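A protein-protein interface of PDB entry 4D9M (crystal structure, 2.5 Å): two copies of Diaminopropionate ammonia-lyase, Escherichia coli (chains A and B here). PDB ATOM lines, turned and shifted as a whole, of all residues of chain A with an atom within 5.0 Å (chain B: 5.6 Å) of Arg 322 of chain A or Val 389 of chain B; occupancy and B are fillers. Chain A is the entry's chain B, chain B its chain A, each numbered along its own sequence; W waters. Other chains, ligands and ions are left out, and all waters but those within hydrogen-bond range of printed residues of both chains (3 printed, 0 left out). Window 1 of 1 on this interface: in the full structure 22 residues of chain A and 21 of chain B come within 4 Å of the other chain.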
ATOM      1  N   ALA A 318     -19.180  17.375  18.788  1.00  0.00           N
ATOM      2  CA  ALA A 318     -19.549  16.726  20.043  1.00  0.00           C
ATOM      3  C   ALA A 318     -20.295  15.423  19.774  1.00  0.00           C
ATOM      4  O   ALA A 318     -20.025  14.401  20.409  1.00  0.00           O
ATOM      5  CB  ALA A 318     -20.381  17.660  20.904  1.00  0.00           C
ATOM      6  N   LEU A 319     -21.221  15.472  18.820  1.00  0.00           N
ATOM      7  CA  LEU A 319     -21.947  14.291  18.369  1.00  0.00           C
ATOM      8  C   LEU A 319     -20.988  13.230  17.824  1.00  0.00           C
ATOM      9  O   LEU A 319     -21.133  12.057  18.133  1.00  0.00           O
ATOM     10  CB  LEU A 319     -22.989  14.680  17.317  1.00  0.00           C
ATOM     11  CG  LEU A 319     -23.789  13.595  16.594  1.00  0.00           C
ATOM     12  CD1 LEU A 319     -24.821  12.949  17.505  1.00  0.00           C
ATOM     13  CD2 LEU A 319     -24.463  14.214  15.379  1.00  0.00           C
ATOM     14  N   GLY A 320     -19.997  13.645  17.042  1.00  0.00           N
ATOM     15  CA  GLY A 320     -18.995  12.720  16.522  1.00  0.00           C
ATOM     16  C   GLY A 320     -18.209  12.023  17.617  1.00  0.00           C
ATOM     17  O   GLY A 320     -17.970  10.807  17.550  1.00  0.00           O
ATOM     18  N   MET A 321     -17.810  12.808  18.620  1.00  0.00           N
ATOM     19  CA  MET A 321     -17.060  12.324  19.776  1.00  0.00           C
ATOM     20  C   MET A 321     -17.812  11.221  20.496  1.00  0.00           C
ATOM     21  O   MET A 321     -17.238  10.173  20.821  1.00  0.00           O
ATOM     22  CB  MET A 321     -16.788  13.464  20.762  1.00  0.00           C
ATOM     23  CG  MET A 321     -15.801  14.511  20.284  1.00  0.00           C
ATOM     24  SD  MET A 321     -15.809  15.923  21.404  1.00  0.00           S
ATOM     25  CE  MET A 321     -14.771  15.303  22.726  1.00  0.00           C
ATOM     26  N   ARG A 322     -19.098  11.468  20.742  1.00  0.00           N
ATOM     27  CA  ARG A 322     -19.950  10.498  21.425  1.00  0.00           C
ATOM     28  C   ARG A 322     -20.194   9.241  20.588  1.00  0.00           C
ATOM     29  O   ARG A 322     -20.256   8.137  21.131  1.00  0.00           O
ATOM     30  CB  ARG A 322     -21.280  11.128  21.840  1.00  0.00           C
ATOM     31  CG  ARG A 322     -21.138  12.253  22.852  1.00  0.00           C
ATOM     32  CD  ARG A 322     -22.471  12.593  23.487  1.00  0.00           C
ATOM     33  NE  ARG A 322     -22.489  13.983  23.914  1.00  0.00           N
ATOM     34  CZ  ARG A 322     -22.881  14.996  23.153  1.00  0.00           C
ATOM     35  NH1 ARG A 322     -23.317  14.787  21.923  1.00  0.00           N
ATOM     36  NH2 ARG A 322     -22.841  16.225  23.628  1.00  0.00           N
ATOM     37  N   VAL A 323     -20.324   9.413  19.275  1.00  0.00           N
ATOM     38  CA  VAL A 323     -20.620   8.291  18.385  1.00  0.00           C
ATOM     39  C   VAL A 323     -19.398   7.381  18.298  1.00  0.00           C
ATOM     40  O   VAL A 323     -19.526   6.155  18.345  1.00  0.00           O
ATOM     41  CB  VAL A 323     -21.106   8.754  16.987  1.00  0.00           C
ATOM     42  CG1 VAL A 323     -21.280   7.567  16.048  1.00  0.00           C
ATOM     43  CG2 VAL A 323     -22.416   9.518  17.101  1.00  0.00           C
ATOM     44  N   LEU A 324     -18.217   7.991  18.232  1.00  0.00           N
ATOM     45  CA  LEU A 324     -16.963   7.247  18.176  1.00  0.00           C
ATOM     46  C   LEU A 324     -16.601   6.524  19.470  1.00  0.00           C
ATOM     47  O   LEU A 324     -16.074   5.414  19.429  1.00  0.00           O
ATOM     48  CB  LEU A 324     -15.811   8.159  17.739  1.00  0.00           C
ATOM     49  CG  LEU A 324     -15.764   8.474  16.239  1.00  0.00           C
ATOM     50  CD1 LEU A 324     -14.790   9.611  15.934  1.00  0.00           C
ATOM     51  CD2 LEU A 324     -15.431   7.231  15.419  1.00  0.00           C
ATOM     52  N   GLY A 325     -16.875   7.164  20.607  1.00  0.00           N
ATOM     53  CA  GLY A 325     -16.516   6.632  21.930  1.00  0.00           C
ATOM     54  C   GLY A 325     -17.510   5.630  22.481  1.00  0.00           C
ATOM     55  O   GLY A 325     -17.198   4.890  23.417  1.00  0.00           O
ATOM     56  N   ASN A 326     -18.716   5.620  21.913  1.00  0.00           N
ATOM     57  CA  ASN A 326     -19.716   4.595  22.218  1.00  0.00           C
ATOM     58  C   ASN A 326     -20.295   4.040  20.918  1.00  0.00           C
ATOM     59  O   ASN A 326     -21.404   4.414  20.513  1.00  0.00           O
ATOM     60  CB  ASN A 326     -20.813   5.143  23.134  1.00  0.00           C
ATOM     61  CG  ASN A 326     -21.642   4.044  23.782  1.00  0.00           C
ATOM     62  OD1 ASN A 326     -21.547   2.866  23.414  1.00  0.00           O
ATOM     63  ND2 ASN A 326     -22.465   4.424  24.759  1.00  0.00           N
ATOM     64  N   VAL A 388     -18.333  16.096  27.291  1.00  0.00           N
ATOM     65  CA  VAL A 388     -19.079  15.738  26.090  1.00  0.00           C
ATOM     66  C   VAL A 388     -19.719  14.347  26.222  1.00  0.00           C
ATOM     67  O   VAL A 388     -20.941  14.218  26.173  1.00  0.00           O
ATOM     68  CB  VAL A 388     -18.188  15.800  24.832  1.00  0.00           C
ATOM     69  CG1 VAL A 388     -19.011  15.523  23.582  1.00  0.00           C
ATOM     70  CG2 VAL A 388     -17.508  17.159  24.720  1.00  0.00           C
ATOM     71  N   VAL A 389     -18.884  13.327  26.424  1.00  0.00           N
ATOM     72  CA  VAL A 389     -19.320  11.924  26.371  1.00  0.00           C
ATOM     73  C   VAL A 389     -20.065  11.419  27.617  1.00  0.00           C
ATOM     74  O   VAL A 389     -20.822  10.449  27.517  1.00  0.00           O
ATOM     75  CB  VAL A 389     -18.162  10.957  25.994  1.00  0.00           C
ATOM     76  CG1 VAL A 389     -17.434  11.458  24.759  1.00  0.00           C
ATOM     77  CG2 VAL A 389     -17.179  10.772  27.145  1.00  0.00           C
ATOM     78  N   GLY A 392     -22.874  15.155  28.626  1.00  0.00           N
ATOM     79  CA  GLY A 392     -23.687  15.607  27.513  1.00  0.00           C
ATOM     80  C   GLY A 392     -23.578  17.096  27.253  1.00  0.00           C
ATOM     81  O   GLY A 392     -24.560  17.730  26.861  1.00  0.00           O
ATOM     82  N   LYS A 393     -22.390  17.661  27.475  1.00  0.00           N
ATOM     83  CA  LYS A 393     -22.103  19.035  27.056  1.00  0.00           C
ATOM     84  C   LYS A 393     -22.204  19.147  25.541  1.00  0.00           C
ATOM     85  O   LYS A 393     -21.818  18.223  24.819  1.00  0.00           O
ATOM     86  CB  LYS A 393     -20.705  19.476  27.496  1.00  0.00           C
ATOM     87  CG  LYS A 393     -20.632  20.092  28.881  1.00  0.00           C
ATOM     88  CD  LYS A 393     -19.514  21.125  28.945  1.00  0.00           C
ATOM     89  N   HIS A 394     -22.714  20.286  25.072  1.00  0.00           N
ATOM     90  CA  HIS A 394     -22.940  20.537  23.642  1.00  0.00           C
ATOM     91  C   HIS A 394     -23.783  19.455  23.032  1.00  0.00           C
ATOM     92  O   HIS A 394     -23.423  18.842  22.029  1.00  0.00           O
ATOM     93  CB  HIS A 394     -21.621  20.759  22.896  1.00  0.00           C
ATOM     94  CG  HIS A 394     -20.780  21.864  23.491  1.00  0.00           C
ATOM     95  ND1 HIS A 394     -19.506  21.678  23.874  1.00  0.00           N
ATOM     96  CD2 HIS A 394     -21.098  23.188  23.804  1.00  0.00           C
ATOM     97  CE1 HIS A 394     -19.022  22.827  24.382  1.00  0.00           C
ATOM     98  NE2 HIS A 394     -20.000  23.749  24.341  1.00  0.00           N
ATOM     99  N   ALA A 395     -24.919  19.218  23.680  1.00  0.00           N
ATOM    100  CA  ALA A 395     -25.903  18.250  23.247  1.00  0.00           C
ATOM    101  C   ALA A 395     -26.670  18.776  22.040  1.00  0.00           C
ATOM    102  O   ALA A 395     -26.675  19.977  21.756  1.00  0.00           O
ATOM    103  CB  ALA A 395     -26.860  17.943  24.388  1.00  0.00           C
ATOM    104  N   MET B 321     -25.593   5.644  32.076  1.00  0.00           N
ATOM    105  CA  MET B 321     -25.576   4.985  30.773  1.00  0.00           C
ATOM    106  C   MET B 321     -24.351   5.402  29.973  1.00  0.00           C
ATOM    107  O   MET B 321     -23.699   4.571  29.332  1.00  0.00           O
ATOM    108  CB  MET B 321     -26.843   5.319  29.975  1.00  0.00           C
ATOM    109  CG  MET B 321     -28.147   4.886  30.617  1.00  0.00           C
ATOM    110  SD  MET B 321     -29.543   5.802  29.938  1.00  0.00           S
ATOM    111  CE  MET B 321     -29.670   5.086  28.299  1.00  0.00           C
ATOM    112  N   ARG B 322     -24.056   6.699  30.012  1.00  0.00           N
ATOM    113  CA  ARG B 322     -22.922   7.266  29.292  1.00  0.00           C
ATOM    114  C   ARG B 322     -21.587   6.825  29.880  1.00  0.00           C
ATOM    115  O   ARG B 322     -20.694   6.437  29.127  1.00  0.00           O
ATOM    116  CB  ARG B 322     -23.022   8.791  29.229  1.00  0.00           C
ATOM    117  CG  ARG B 322     -24.251   9.284  28.479  1.00  0.00           C
ATOM    118  CD  ARG B 322     -24.144  10.748  28.085  1.00  0.00           C
ATOM    119  NE  ARG B 322     -25.469  11.351  28.027  1.00  0.00           N
ATOM    120  CZ  ARG B 322     -26.008  12.064  29.008  1.00  0.00           C
ATOM    121  NH1 ARG B 322     -25.324  12.289  30.119  1.00  0.00           N
ATOM    122  NH2 ARG B 322     -27.232  12.556  28.875  1.00  0.00           N
ATOM    123  N   ASN B 326     -19.247   4.427  27.607  1.00  0.00           N
ATOM    124  CA  ASN B 326     -17.942   4.964  27.228  1.00  0.00           C
ATOM    125  C   ASN B 326     -17.049   4.983  28.474  1.00  0.00           C
ATOM    126  O   ASN B 326     -16.988   5.984  29.183  1.00  0.00           O
ATOM    127  CB  ASN B 326     -18.088   6.363  26.616  1.00  0.00           C
ATOM    128  CG  ASN B 326     -16.823   6.848  25.915  1.00  0.00           C
ATOM    129  OD1 ASN B 326     -15.733   6.296  26.089  1.00  0.00           O
ATOM    130  ND2 ASN B 326     -16.968   7.894  25.116  1.00  0.00           N
ATOM    131  N   HIS B 384     -33.944   5.341  22.421  1.00  0.00           N
ATOM    132  CA  HIS B 384     -33.687   6.119  23.622  1.00  0.00           C
ATOM    133  C   HIS B 384     -32.250   6.005  24.057  1.00  0.00           C
ATOM    134  O   HIS B 384     -31.629   7.014  24.407  1.00  0.00           O
ATOM    135  CB  HIS B 384     -34.638   5.712  24.743  1.00  0.00           C
ATOM    136  CG  HIS B 384     -34.528   6.573  25.979  1.00  0.00           C
ATOM    137  ND1 HIS B 384     -34.898   7.869  25.996  1.00  0.00           N
ATOM    138  CD2 HIS B 384     -34.069   6.278  27.264  1.00  0.00           C
ATOM    139  CE1 HIS B 384     -34.689   8.380  27.226  1.00  0.00           C
ATOM    140  NE2 HIS B 384     -34.183   7.405  28.003  1.00  0.00           N
ATOM    141  N   TYR B 385     -31.702   4.790  24.018  1.00  0.00           N
ATOM    142  CA  TYR B 385     -30.309   4.564  24.396  1.00  0.00           C
ATOM    143  C   TYR B 385     -29.335   5.445  23.613  1.00  0.00           C
ATOM    144  O   TYR B 385     -28.408   6.022  24.192  1.00  0.00           O
ATOM    145  CB  TYR B 385     -29.905   3.089  24.248  1.00  0.00           C
ATOM    146  CG  TYR B 385     -28.471   2.843  24.657  1.00  0.00           C
ATOM    147  CD1 TYR B 385     -28.117   2.744  26.007  1.00  0.00           C
ATOM    148  CD2 TYR B 385     -27.456   2.752  23.706  1.00  0.00           C
ATOM    149  CE1 TYR B 385     -26.798   2.542  26.395  1.00  0.00           C
ATOM    150  CE2 TYR B 385     -26.134   2.550  24.085  1.00  0.00           C
ATOM    151  CZ  TYR B 385     -25.810   2.444  25.430  1.00  0.00           C
ATOM    152  OH  TYR B 385     -24.496   2.242  25.819  1.00  0.00           O
ATOM    153  N   ARG B 386     -29.549   5.547  22.301  1.00  0.00           N
ATOM    154  CA  ARG B 386     -28.638   6.300  21.444  1.00  0.00           C
ATOM    155  C   ARG B 386     -28.921   7.792  21.514  1.00  0.00           C
ATOM    156  O   ARG B 386     -28.017   8.600  21.313  1.00  0.00           O
ATOM    157  CB  ARG B 386     -28.667   5.786  19.997  1.00  0.00           C
ATOM    158  CG  ARG B 386     -28.143   4.367  19.837  1.00  0.00           C
ATOM    159  CD  ARG B 386     -26.663   4.269  20.170  1.00  0.00           C
ATOM    160  NE  ARG B 386     -26.200   2.887  20.210  1.00  0.00           N
ATOM    161  CZ  ARG B 386     -24.958   2.512  20.503  1.00  0.00           C
ATOM    162  NH1 ARG B 386     -24.030   3.419  20.792  1.00  0.00           N
ATOM    163  NH2 ARG B 386     -24.643   1.226  20.513  1.00  0.00           N
ATOM    164  N   GLU B 387     -30.170   8.155  21.810  1.00  0.00           N
ATOM    165  CA  GLU B 387     -30.506   9.555  22.091  1.00  0.00           C
ATOM    166  C   GLU B 387     -29.778  10.074  23.341  1.00  0.00           C
ATOM    167  O   GLU B 387     -29.347  11.229  23.382  1.00  0.00           O
ATOM    168  CB  GLU B 387     -32.018   9.753  22.234  1.00  0.00           C
ATOM    169  CG  GLU B 387     -32.750   9.949  20.913  1.00  0.00           C
ATOM    170  CD  GLU B 387     -34.233   9.630  21.000  1.00  0.00           C
ATOM    171  OE1 GLU B 387     -34.725   9.372  22.116  1.00  0.00           O
ATOM    172  OE2 GLU B 387     -34.912   9.633  19.948  1.00  0.00           O
ATOM    173  N   VAL B 388     -29.638   9.215  24.348  1.00  0.00           N
ATOM    174  CA  VAL B 388     -28.932   9.581  25.574  1.00  0.00           C
ATOM    175  C   VAL B 388     -27.413   9.642  25.366  1.00  0.00           C
ATOM    176  O   VAL B 388     -26.783  10.655  25.676  1.00  0.00           O
ATOM    177  CB  VAL B 388     -29.283   8.629  26.744  1.00  0.00           C
ATOM    178  CG1 VAL B 388     -28.346   8.846  27.930  1.00  0.00           C
ATOM    179  CG2 VAL B 388     -30.734   8.808  27.167  1.00  0.00           C
ATOM    180  N   VAL B 389     -26.836   8.568  24.821  1.00  0.00           N
ATOM    181  CA  VAL B 389     -25.376   8.438  24.726  1.00  0.00           C
ATOM    182  C   VAL B 389     -24.722   9.159  23.541  1.00  0.00           C
ATOM    183  O   VAL B 389     -23.538   9.506  23.622  1.00  0.00           O
ATOM    184  CB  VAL B 389     -24.887   6.962  24.792  1.00  0.00           C
ATOM    185  CG1 VAL B 389     -25.422   6.266  26.033  1.00  0.00           C
ATOM    186  CG2 VAL B 389     -25.247   6.194  23.523  1.00  0.00           C
ATOM    187  N   TRP B 390     -25.473   9.382  22.458  1.00  0.00           N
ATOM    188  CA  TRP B 390     -24.963  10.140  21.299  1.00  0.00           C
ATOM    189  C   TRP B 390     -25.446  11.566  21.231  1.00  0.00           C
ATOM    190  O   TRP B 390     -24.658  12.483  20.969  1.00  0.00           O
ATOM    191  CB  TRP B 390     -25.298   9.456  19.976  1.00  0.00           C
ATOM    192  CG  TRP B 390     -24.605   8.139  19.715  1.00  0.00           C
ATOM    193  CD1 TRP B 390     -23.587   7.548  20.451  1.00  0.00           C
ATOM    194  CD2 TRP B 390     -24.845   7.222  18.589  1.00  0.00           C
ATOM    195  NE1 TRP B 390     -23.207   6.353  19.892  1.00  0.00           N
ATOM    196  CE2 TRP B 390     -23.917   6.100  18.770  1.00  0.00           C
ATOM    197  CE3 TRP B 390     -25.707   7.218  17.492  1.00  0.00           C
ATOM    198  CZ2 TRP B 390     -23.872   5.030  17.880  1.00  0.00           C
ATOM    199  CZ3 TRP B 390     -25.654   6.136  16.607  1.00  0.00           C
ATOM    200  CH2 TRP B 390     -24.756   5.070  16.796  1.00  0.00           C
ATOM    201  N   GLU B 391     -26.746  11.771  21.435  1.00  0.00           N
ATOM    202  CA  GLU B 391     -27.346  13.096  21.286  1.00  0.00           C
ATOM    203  C   GLU B 391     -27.219  13.882  22.584  1.00  0.00           C
ATOM    204  O   GLU B 391     -27.310  15.116  22.595  1.00  0.00           O
ATOM    205  CB  GLU B 391     -28.816  12.993  20.846  1.00  0.00           C
ATOM    206  CG  GLU B 391     -29.023  12.336  19.484  1.00  0.00           C
ATOM    207  CD  GLU B 391     -30.482  12.042  19.148  1.00  0.00           C
ATOM    208  OE1 GLU B 391     -31.392  12.767  19.614  1.00  0.00           O
ATOM    209  OE2 GLU B 391     -30.723  11.079  18.385  1.00  0.00           O
ATOM    210  N   GLY B 392     -26.996  13.164  23.679  1.00  0.00           N
ATOM    211  CA  GLY B 392     -26.930  13.794  24.984  1.00  0.00           C
ATOM    212  C   GLY B 392     -28.268  14.356  25.421  1.00  0.00           C
ATOM    213  O   GLY B 392     -28.337  15.463  25.965  1.00  0.00           O
HETATM  214  O   HOH W   1     -21.434   8.676  25.347  1.00  0.00           O
HETATM  215  O   HOH W   2     -21.551   6.435  26.301  1.00  0.00           O
HETATM  216  O   HOH W   3     -19.352   8.515  23.865  1.00  0.00           O
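Arg 322 of chain A touches Val 389 of chain B, and with the chains exchanged Val 389 of chain A touches Arg 322 of chain B. Asn 326 of chain A touches Val 389 of chain B, and with the chains exchanged Val 389 of chain A touches Asn 326 of chain B. 6 positions are printed for both chains. Of the 13 pairs that touch across the chains among the printed residues, 4 have their exchanged pair printed and touching as well.
Arg 322 of chain A touches just these residues of chain B: Val 389 and Trp 390. Of the printed residues of chain A, Arg 322 of chain B touches Val 389. Printed residues of chain A within 4 Å of Arg 386 of chain B: Asn 326 (2.8 Å). Of chain A, only Arg 322 and Asn 326 come within 4 Å of Val 389 of chain B. The nearest residue of chain A that does not touch Val 389 of chain B is Val 389 of chain A (4.8 Å).
Water W2 lies within hydrogen-bond range of the side-chain amide nitrogen of Asn 326 of chain A, the backbone carbonyl oxygen of Arg 322 of chain B and the backbone NH of Asn 326 of chain B. Water W3 bridges ND2 of Asn 326 of chain B and O of Arg 322 of chain A. Water W1 bridges the backbone carbonyl oxygen (O) of Val 389 of chain B (2.8 Å) and the backbone carbonyl oxygen (O) of Val 389 of chain A (2.9 Å).
N of Gly 392 of chain B lies within hydrogen-bond range of O of Glu 387 of chain B (3.1 Å). NE of Arg 322 of chain B lies within hydrogen-bond range of O of Val 388 of chain B, 2.8 Å away. The backbone carbonyl oxygen (O) of His 394 of chain A is in hydrogen-bond range of the guanidinium group (NH2) of Arg 322 of chain A, at 3.1 Å. The guanidinium group of Arg 322 of chain A sits at hydrogen-bond distance from the backbone carbonyl oxygen of Lys 393 of chain A, at 2.5 Å. O of Val 388 of chain A is in hydrogen-bond range of NE of Arg 322 of chain A (2.7 Å). The backbone NH (N) of Glu 391 of chain B is in hydrogen-bond range of the backbone carbonyl oxygen (O) of Arg 386 of chain B, 3.4 Å away.
Trp 390 of chain B touches Leu 319 of chain A. CD of Arg 322 of chain A touches O of Val 389 of chain B (3.3 Å). NE1 of Trp 390 of chain B touches CA of Val 323 of chain A, at 3.6 Å. ND2 of Asn 326 of chain A touches CB of Val 389 of chain B (3.5 Å). Arg 322 of chain B touches Val 389 of chain A (CB to O, 3.2 Å). Asn 326 of chain B touches Val 389 of chain A. O of Glu 391 of chain B touches CB of Ala 395 of chain A (3.4 Å). Gly 392 of chain B touches Ala 395 of chain A (O to CB, 3.3 Å).
OH of Tyr 385 of chain B is in hydrogen-bond range of ND2 of Asn 326 of chain A, at 3.2 Å. O of Asn 326 of chain A lies within hydrogen-bond range of NH1 of Arg 386 of chain B. NE1 of Trp 390 of chain B lies within hydrogen-bond range of O of Asn 326 of chain A (2.7 Å). The backbone carbonyl oxygen (O) of Trp 390 of chain B lies within hydrogen-bond range of the guanidinium group (NH1) of Arg 322 of chain A. The side-chain amide oxygen (OD1) of Asn 326 of chain B lies close to the backbone carbonyl oxygen (O) of Gly 325 of chain A (3.4 Å).
Along chain A the printed residues that touch a printed residue of chain B span positions 319 to 395. Among the printed residues, no Asp or Glu carboxylate lies within 4 Å of a Lys or Arg side-chain nitrogen of the other chain.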
